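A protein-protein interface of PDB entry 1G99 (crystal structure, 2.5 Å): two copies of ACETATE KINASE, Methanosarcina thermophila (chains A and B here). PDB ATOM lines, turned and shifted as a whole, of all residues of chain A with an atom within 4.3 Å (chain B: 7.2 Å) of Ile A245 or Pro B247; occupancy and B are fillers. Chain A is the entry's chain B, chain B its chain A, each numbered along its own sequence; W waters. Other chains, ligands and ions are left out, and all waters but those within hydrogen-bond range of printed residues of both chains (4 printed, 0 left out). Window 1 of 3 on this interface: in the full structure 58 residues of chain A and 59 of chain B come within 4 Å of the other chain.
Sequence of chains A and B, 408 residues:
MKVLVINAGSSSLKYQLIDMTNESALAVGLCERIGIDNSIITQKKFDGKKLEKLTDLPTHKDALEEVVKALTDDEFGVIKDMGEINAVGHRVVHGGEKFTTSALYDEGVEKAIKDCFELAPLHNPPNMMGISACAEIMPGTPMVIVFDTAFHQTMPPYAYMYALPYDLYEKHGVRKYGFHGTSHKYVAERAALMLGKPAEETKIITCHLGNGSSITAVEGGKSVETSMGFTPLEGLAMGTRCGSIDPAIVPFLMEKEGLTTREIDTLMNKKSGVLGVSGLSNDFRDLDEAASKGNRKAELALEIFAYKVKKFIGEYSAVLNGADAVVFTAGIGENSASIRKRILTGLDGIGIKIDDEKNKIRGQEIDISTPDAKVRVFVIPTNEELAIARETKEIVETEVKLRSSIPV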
ATOM      1  N   LEU A 233       2.470  25.534  12.092  1.00  0.00           N
ATOM      2  CA  LEU A 233       3.234  26.681  11.581  1.00  0.00           C
ATOM      3  C   LEU A 233       4.264  26.384  10.496  1.00  0.00           C
ATOM      4  O   LEU A 233       4.576  27.245   9.669  1.00  0.00           O
ATOM      5  CB  LEU A 233       3.950  27.395  12.730  1.00  0.00           C
ATOM      6  CG  LEU A 233       4.900  28.548  12.356  1.00  0.00           C
ATOM      7  CD1 LEU A 233       4.125  29.690  11.668  1.00  0.00           C
ATOM      8  CD2 LEU A 233       5.593  29.078  13.627  1.00  0.00           C
ATOM      9  N   CYS A 242       3.970  32.472   8.921  1.00  0.00           N
ATOM     10  CA  CYS A 242       5.206  32.646   8.171  1.00  0.00           C
ATOM     11  C   CYS A 242       5.765  31.388   7.523  1.00  0.00           C
ATOM     12  O   CYS A 242       6.465  31.468   6.530  1.00  0.00           O
ATOM     13  CB  CYS A 242       6.271  33.288   9.068  1.00  0.00           C
ATOM     14  SG  CYS A 242       6.874  32.258  10.483  1.00  0.00           S
ATOM     15  N   GLY A 243       5.441  30.224   8.057  1.00  0.00           N
ATOM     16  CA  GLY A 243       5.958  29.017   7.477  1.00  0.00           C
ATOM     17  C   GLY A 243       7.400  28.842   7.903  1.00  0.00           C
ATOM     18  O   GLY A 243       7.861  29.466   8.862  1.00  0.00           O
ATOM     19  N   SER A 244       8.116  27.997   7.178  1.00  0.00           N
ATOM     20  CA  SER A 244       9.518  27.705   7.447  1.00  0.00           C
ATOM     21  C   SER A 244      10.501  28.813   7.095  1.00  0.00           C
ATOM     22  O   SER A 244      10.873  28.974   5.945  1.00  0.00           O
ATOM     23  CB  SER A 244       9.936  26.431   6.702  1.00  0.00           C
ATOM     24  OG  SER A 244       9.158  25.325   7.104  1.00  0.00           O
ATOM     25  N   ILE A 245      10.953  29.545   8.097  1.00  0.00           N
ATOM     26  CA  ILE A 245      11.909  30.628   7.895  1.00  0.00           C
ATOM     27  C   ILE A 245      13.225  30.183   8.507  1.00  0.00           C
ATOM     28  O   ILE A 245      13.297  29.117   9.093  1.00  0.00           O
ATOM     29  CB  ILE A 245      11.463  31.900   8.654  1.00  0.00           C
ATOM     30  CG1 ILE A 245      11.391  31.587  10.160  1.00  0.00           C
ATOM     31  CG2 ILE A 245      10.137  32.382   8.114  1.00  0.00           C
ATOM     32  CD1 ILE A 245      10.888  32.731  11.008  1.00  0.00           C
ATOM     33  N   ASP A 246      14.271  30.993   8.388  1.00  0.00           N
ATOM     34  CA  ASP A 246      15.554  30.641   9.012  1.00  0.00           C
ATOM     35  C   ASP A 246      15.265  30.687  10.528  1.00  0.00           C
ATOM     36  O   ASP A 246      14.896  31.726  11.051  1.00  0.00           O
ATOM     37  CB  ASP A 246      16.612  31.687   8.654  1.00  0.00           C
ATOM     38  CG  ASP A 246      17.952  31.452   9.351  1.00  0.00           C
ATOM     39  OD1 ASP A 246      18.029  30.643  10.292  1.00  0.00           O
ATOM     40  OD2 ASP A 246      18.947  32.096   8.964  1.00  0.00           O
ATOM     41  N   PRO A 247      15.418  29.557  11.245  1.00  0.00           N
ATOM     42  CA  PRO A 247      15.155  29.523  12.683  1.00  0.00           C
ATOM     43  C   PRO A 247      15.961  30.548  13.495  1.00  0.00           C
ATOM     44  O   PRO A 247      15.573  30.921  14.598  1.00  0.00           O
ATOM     45  CB  PRO A 247      15.532  28.097  13.067  1.00  0.00           C
ATOM     46  CG  PRO A 247      15.391  27.346  11.811  1.00  0.00           C
ATOM     47  CD  PRO A 247      15.928  28.256  10.792  1.00  0.00           C
ATOM     48  N   ILE A 249      16.247  33.521  12.941  1.00  0.00           N
ATOM     49  CA  ILE A 249      15.508  34.779  12.958  1.00  0.00           C
ATOM     50  C   ILE A 249      14.728  34.916  14.260  1.00  0.00           C
ATOM     51  O   ILE A 249      14.449  36.025  14.724  1.00  0.00           O
ATOM     52  CB  ILE A 249      14.520  34.867  11.754  1.00  0.00           C
ATOM     53  CG1 ILE A 249      15.315  34.980  10.439  1.00  0.00           C
ATOM     54  CG2 ILE A 249      13.558  36.047  11.932  1.00  0.00           C
ATOM     55  CD1 ILE A 249      14.420  34.886   9.195  1.00  0.00           C
ATOM     56  N   MET A 268       4.689  35.224  14.682  1.00  0.00           N
ATOM     57  CA  MET A 268       4.818  34.210  13.642  1.00  0.00           C
ATOM     58  C   MET A 268       3.490  33.581  13.197  1.00  0.00           C
ATOM     59  O   MET A 268       3.343  33.222  12.041  1.00  0.00           O
ATOM     60  CB  MET A 268       5.789  33.090  14.088  1.00  0.00           C
ATOM     61  CG  MET A 268       7.216  33.567  14.230  1.00  0.00           C
ATOM     62  SD  MET A 268       8.346  32.214  14.383  1.00  0.00           S
ATOM     63  CE  MET A 268       7.910  31.512  16.026  1.00  0.00           C
ATOM     64  N   TYR B 162      11.079  36.782   3.342  1.00  0.00           N
ATOM     65  CA  TYR B 162      10.400  35.801   4.178  1.00  0.00           C
ATOM     66  C   TYR B 162       8.955  36.305   4.317  1.00  0.00           C
ATOM     67  O   TYR B 162       8.710  37.500   4.184  1.00  0.00           O
ATOM     68  CB  TYR B 162      11.024  35.748   5.558  1.00  0.00           C
ATOM     69  CG  TYR B 162      12.368  35.095   5.553  1.00  0.00           C
ATOM     70  CD1 TYR B 162      12.490  33.702   5.432  1.00  0.00           C
ATOM     71  CD2 TYR B 162      13.539  35.862   5.651  1.00  0.00           C
ATOM     72  CE1 TYR B 162      13.733  33.093   5.409  1.00  0.00           C
ATOM     73  CE2 TYR B 162      14.792  35.266   5.627  1.00  0.00           C
ATOM     74  CZ  TYR B 162      14.878  33.884   5.507  1.00  0.00           C
ATOM     75  OH  TYR B 162      16.110  33.308   5.487  1.00  0.00           O
ATOM     76  N   ALA B 163       8.007  35.405   4.575  1.00  0.00           N
ATOM     77  CA  ALA B 163       6.621  35.817   4.744  1.00  0.00           C
ATOM     78  C   ALA B 163       6.419  36.314   6.195  1.00  0.00           C
ATOM     79  O   ALA B 163       5.659  35.746   6.978  1.00  0.00           O
ATOM     80  CB  ALA B 163       5.690  34.659   4.418  1.00  0.00           C
ATOM     81  N   LEU B 164       7.151  37.362   6.536  1.00  0.00           N
ATOM     82  CA  LEU B 164       7.108  37.995   7.851  1.00  0.00           C
ATOM     83  C   LEU B 164       6.600  39.423   7.640  1.00  0.00           C
ATOM     84  O   LEU B 164       6.459  39.876   6.491  1.00  0.00           O
ATOM     85  CB  LEU B 164       8.511  38.059   8.459  1.00  0.00           C
ATOM     86  CG  LEU B 164       9.036  36.742   9.028  1.00  0.00           C
ATOM     87  CD1 LEU B 164      10.528  36.854   9.292  1.00  0.00           C
ATOM     88  CD2 LEU B 164       8.257  36.388  10.298  1.00  0.00           C
ATOM     89  N   GLU B 234      19.888  28.128   8.030  1.00  0.00           N
ATOM     90  CA  GLU B 234      18.742  27.664   7.262  1.00  0.00           C
ATOM     91  C   GLU B 234      18.991  26.555   6.246  1.00  0.00           C
ATOM     92  O   GLU B 234      20.085  26.445   5.683  1.00  0.00           O
ATOM     93  CB  GLU B 234      18.089  28.853   6.550  1.00  0.00           C
ATOM     94  CG  GLU B 234      16.839  28.505   5.761  1.00  0.00           C
ATOM     95  CD  GLU B 234      16.045  29.743   5.331  1.00  0.00           C
ATOM     96  OE1 GLU B 234      16.500  30.886   5.538  1.00  0.00           O
ATOM     97  OE2 GLU B 234      14.959  29.567   4.778  1.00  0.00           O
ATOM     98  N   GLY B 235      17.956  25.748   6.006  1.00  0.00           N
ATOM     99  CA  GLY B 235      18.071  24.700   5.004  1.00  0.00           C
ATOM    100  C   GLY B 235      18.301  23.268   5.438  1.00  0.00           C
ATOM    101  O   GLY B 235      17.484  22.681   6.147  1.00  0.00           O
ATOM    102  N   GLY B 243      19.242  23.180  10.656  1.00  0.00           N
ATOM    103  CA  GLY B 243      18.591  23.510   9.403  1.00  0.00           C
ATOM    104  C   GLY B 243      17.179  24.014   9.665  1.00  0.00           C
ATOM    105  O   GLY B 243      16.836  24.440  10.777  1.00  0.00           O
ATOM    106  N   SER B 244      16.346  23.948   8.640  1.00  0.00           N
ATOM    107  CA  SER B 244      14.963  24.400   8.719  1.00  0.00           C
ATOM    108  C   SER B 244      13.977  23.525   9.510  1.00  0.00           C
ATOM    109  O   SER B 244      13.403  22.589   8.984  1.00  0.00           O
ATOM    110  CB  SER B 244      14.434  24.584   7.298  1.00  0.00           C
ATOM    111  OG  SER B 244      15.176  25.570   6.616  1.00  0.00           O
ATOM    112  N   ILE B 245      13.744  23.858  10.762  1.00  0.00           N
ATOM    113  CA  ILE B 245      12.812  23.115  11.595  1.00  0.00           C
ATOM    114  C   ILE B 245      11.541  23.929  11.732  1.00  0.00           C
ATOM    115  O   ILE B 245      11.463  25.031  11.218  1.00  0.00           O
ATOM    116  CB  ILE B 245      13.409  22.935  12.982  1.00  0.00           C
ATOM    117  CG1 ILE B 245      13.689  24.331  13.604  1.00  0.00           C
ATOM    118  CG2 ILE B 245      14.680  22.074  12.886  1.00  0.00           C
ATOM    119  CD1 ILE B 245      14.380  24.250  14.955  1.00  0.00           C
ATOM    120  N   ASP B 246      10.533  23.393  12.401  1.00  0.00           N
ATOM    121  CA  ASP B 246       9.315  24.173  12.632  1.00  0.00           C
ATOM    122  C   ASP B 246       9.802  25.330  13.551  1.00  0.00           C
ATOM    123  O   ASP B 246      10.339  25.078  14.621  1.00  0.00           O
ATOM    124  CB  ASP B 246       8.286  23.312  13.377  1.00  0.00           C
ATOM    125  CG  ASP B 246       7.027  24.088  13.749  1.00  0.00           C
ATOM    126  OD1 ASP B 246       7.030  25.328  13.657  1.00  0.00           O
ATOM    127  OD2 ASP B 246       6.033  23.457  14.151  1.00  0.00           O
ATOM    128  N   PRO B 247       9.652  26.596  13.123  1.00  0.00           N
ATOM    129  CA  PRO B 247      10.097  27.746  13.933  1.00  0.00           C
ATOM    130  C   PRO B 247       9.422  27.800  15.308  1.00  0.00           C
ATOM    131  O   PRO B 247       9.975  28.369  16.221  1.00  0.00           O
ATOM    132  CB  PRO B 247       9.727  28.956  13.076  1.00  0.00           C
ATOM    133  CG  PRO B 247       9.621  28.409  11.715  1.00  0.00           C
ATOM    134  CD  PRO B 247       9.029  27.043  11.871  1.00  0.00           C
ATOM    135  N   ALA B 248       8.233  27.208  15.446  1.00  0.00           N
ATOM    136  CA  ALA B 248       7.526  27.203  16.724  1.00  0.00           C
ATOM    137  C   ALA B 248       8.301  26.427  17.801  1.00  0.00           C
ATOM    138  O   ALA B 248       8.105  26.659  18.999  1.00  0.00           O
ATOM    139  CB  ALA B 248       6.150  26.616  16.544  1.00  0.00           C
ATOM    140  N   ILE B 249       9.181  25.515  17.371  1.00  0.00           N
ATOM    141  CA  ILE B 249      10.001  24.743  18.304  1.00  0.00           C
ATOM    142  C   ILE B 249      10.916  25.673  19.125  1.00  0.00           C
ATOM    143  O   ILE B 249      11.264  25.359  20.250  1.00  0.00           O
ATOM    144  CB  ILE B 249      10.884  23.710  17.552  1.00  0.00           C
ATOM    145  CG1 ILE B 249       9.982  22.620  16.948  1.00  0.00           C
ATOM    146  CG2 ILE B 249      11.946  23.121  18.488  1.00  0.00           C
ATOM    147  CD1 ILE B 249      10.704  21.705  15.984  1.00  0.00           C
ATOM    148  N   VAL B 250      11.290  26.828  18.579  1.00  0.00           N
ATOM    149  CA  VAL B 250      12.175  27.703  19.333  1.00  0.00           C
ATOM    150  C   VAL B 250      11.509  28.244  20.601  1.00  0.00           C
ATOM    151  O   VAL B 250      11.999  27.995  21.703  1.00  0.00           O
ATOM    152  CB  VAL B 250      12.701  28.840  18.452  1.00  0.00           C
ATOM    153  CG1 VAL B 250      13.588  29.753  19.269  1.00  0.00           C
ATOM    154  CG2 VAL B 250      13.480  28.242  17.266  1.00  0.00           C
ATOM    155  N   PRO B 251      10.367  28.958  20.480  1.00  0.00           N
ATOM    156  CA  PRO B 251       9.761  29.451  21.726  1.00  0.00           C
ATOM    157  C   PRO B 251       9.381  28.314  22.684  1.00  0.00           C
ATOM    158  O   PRO B 251       9.543  28.408  23.905  1.00  0.00           O
ATOM    159  CB  PRO B 251       8.555  30.278  21.241  1.00  0.00           C
ATOM    160  CG  PRO B 251       8.269  29.781  19.879  1.00  0.00           C
ATOM    161  CD  PRO B 251       9.624  29.447  19.300  1.00  0.00           C
ATOM    162  N   PHE B 252       8.910  27.222  22.113  1.00  0.00           N
ATOM    163  CA  PHE B 252       8.526  26.050  22.883  1.00  0.00           C
ATOM    164  C   PHE B 252       9.682  25.518  23.751  1.00  0.00           C
ATOM    165  O   PHE B 252       9.513  25.269  24.943  1.00  0.00           O
ATOM    166  CB  PHE B 252       8.065  24.959  21.925  1.00  0.00           C
ATOM    167  CG  PHE B 252       7.813  23.614  22.587  1.00  0.00           C
ATOM    168  CD1 PHE B 252       6.585  23.330  23.189  1.00  0.00           C
ATOM    169  CD2 PHE B 252       8.802  22.654  22.618  1.00  0.00           C
ATOM    170  CE1 PHE B 252       6.349  22.102  23.811  1.00  0.00           C
ATOM    171  CE2 PHE B 252       8.585  21.417  23.245  1.00  0.00           C
ATOM    172  CZ  PHE B 252       7.355  21.138  23.844  1.00  0.00           C
HETATM  173  O   HOH W   1      10.806  23.073   7.520  1.00  0.00           O
HETATM  174  O   HOH W   2      12.397  26.772   8.979  1.00  0.00           O
HETATM  175  O   HOH W   3       8.641  32.690   4.808  1.00  0.00           O
HETATM  176  O   HOH W   4      13.481  27.428   5.296  1.00  0.00           O
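The backbone NH (N) of Cys A242 lies within hydrogen-bond range of the backbone carbonyl oxygen (O) of Met A268 (3.3 Å).
The backbone carbonyl oxygen (O) of Leu A233 sits close to the backbone NH (N) of Gly A243, at 3.5 Å.
The side-chain hydroxyl (OH) of Tyr B162 is in hydrogen-bond range of the side-chain carboxylate (OE1) of Glu B234 (2.5 Å).
N of Ala B248 sits at hydrogen-bond distance from OD1 of Asp B246, 2.9 Å away.
Gly A243 touches Pro B247, and with the chains exchanged Pro A247 touches Gly B243.
Ile A245 touches Pro B247, and with the chains exchanged Pro A247 touches Ile B245.
Of the 13 pairs that touch across the chains among the printed residues, 4 have their exchanged pair printed and touching as well.
Hydrophobic or aromatic side chains of chain A within 4 Å of the printed part of chain B: Leu A233, Ile A245, Pro A247, Ile A249 and Met A268.
Of the 15 printed residues of chain B, 9 touch a printed residue of chain A.
Hydrophobic or aromatic side chains of chain B within 4 Å of the printed part of chain A: Tyr B162, Ala B163, Leu B164, Ile B245, Pro B247 and Ala B248.
Among the printed residues, no Asp or Glu carboxylate lies within 4 Å of a Lys or Arg side-chain nitrogen of the other chain.
Among the printed residues, merely in contact across the chains: Leu A233 with Asp B246 (3.8 Å), Leu A233 with Ala B248 (3.7 Å), Cys A242 with Ala B163 (3.3 Å), Cys A242 with Leu B164 (3.9 Å), Gly A243 with Pro B247 (3.5 Å), Ile A245 with Tyr B162 (3.8 Å), Ile A245 with Pro B247 (3.96 Å), Asp A246 with Tyr B162 (3.6 Å), Asp A246 with Glu B234 (3.2 Å), Pro A247 with Gly B243 (3.4 Å), Pro A247 with Ile B245 (3.9 Å), Ile A249 with Tyr B162 (3.6 Å) and Met A268 with Pro B247 (3.8 Å).
Water W2 lies within hydrogen-bond range of O of Ile A245 and O of Ile B245.
Water W4 lies within hydrogen-bond range of OE2 of Glu B234 (2.7 Å), OG of Ser B244 (2.8 Å) and O of Ser A244 (3.1 Å).
Water W3 bridges the backbone NH of Ala B163 and the backbone carbonyl oxygen of Cys A242.
Water W1 lies within hydrogen-bond range of OG of Ser A244 (2.8 Å) and O of Ser B244 (3.0 Å).
Of chain B, only Tyr B162 and Pro B247 come within 4 Å of Ile A245.
Of the printed residues of chain A, Pro B247 touches Gly A243, Ile A245 and Met A268.
Of the printed residues of chain B, Cys A242 touches Ala B163 and Leu B164.
Of the printed residues of chain A, Ile B245 touches Pro A247.
Ser A244 touches none of the printed residues of chain B.
The nearest residue of chain B that does not touch Ile A245 is Glu B234 (4.2 Å).
The nearest printed residue of chain A that does not touch Tyr B162 is Ser A244 (5.0 Å).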
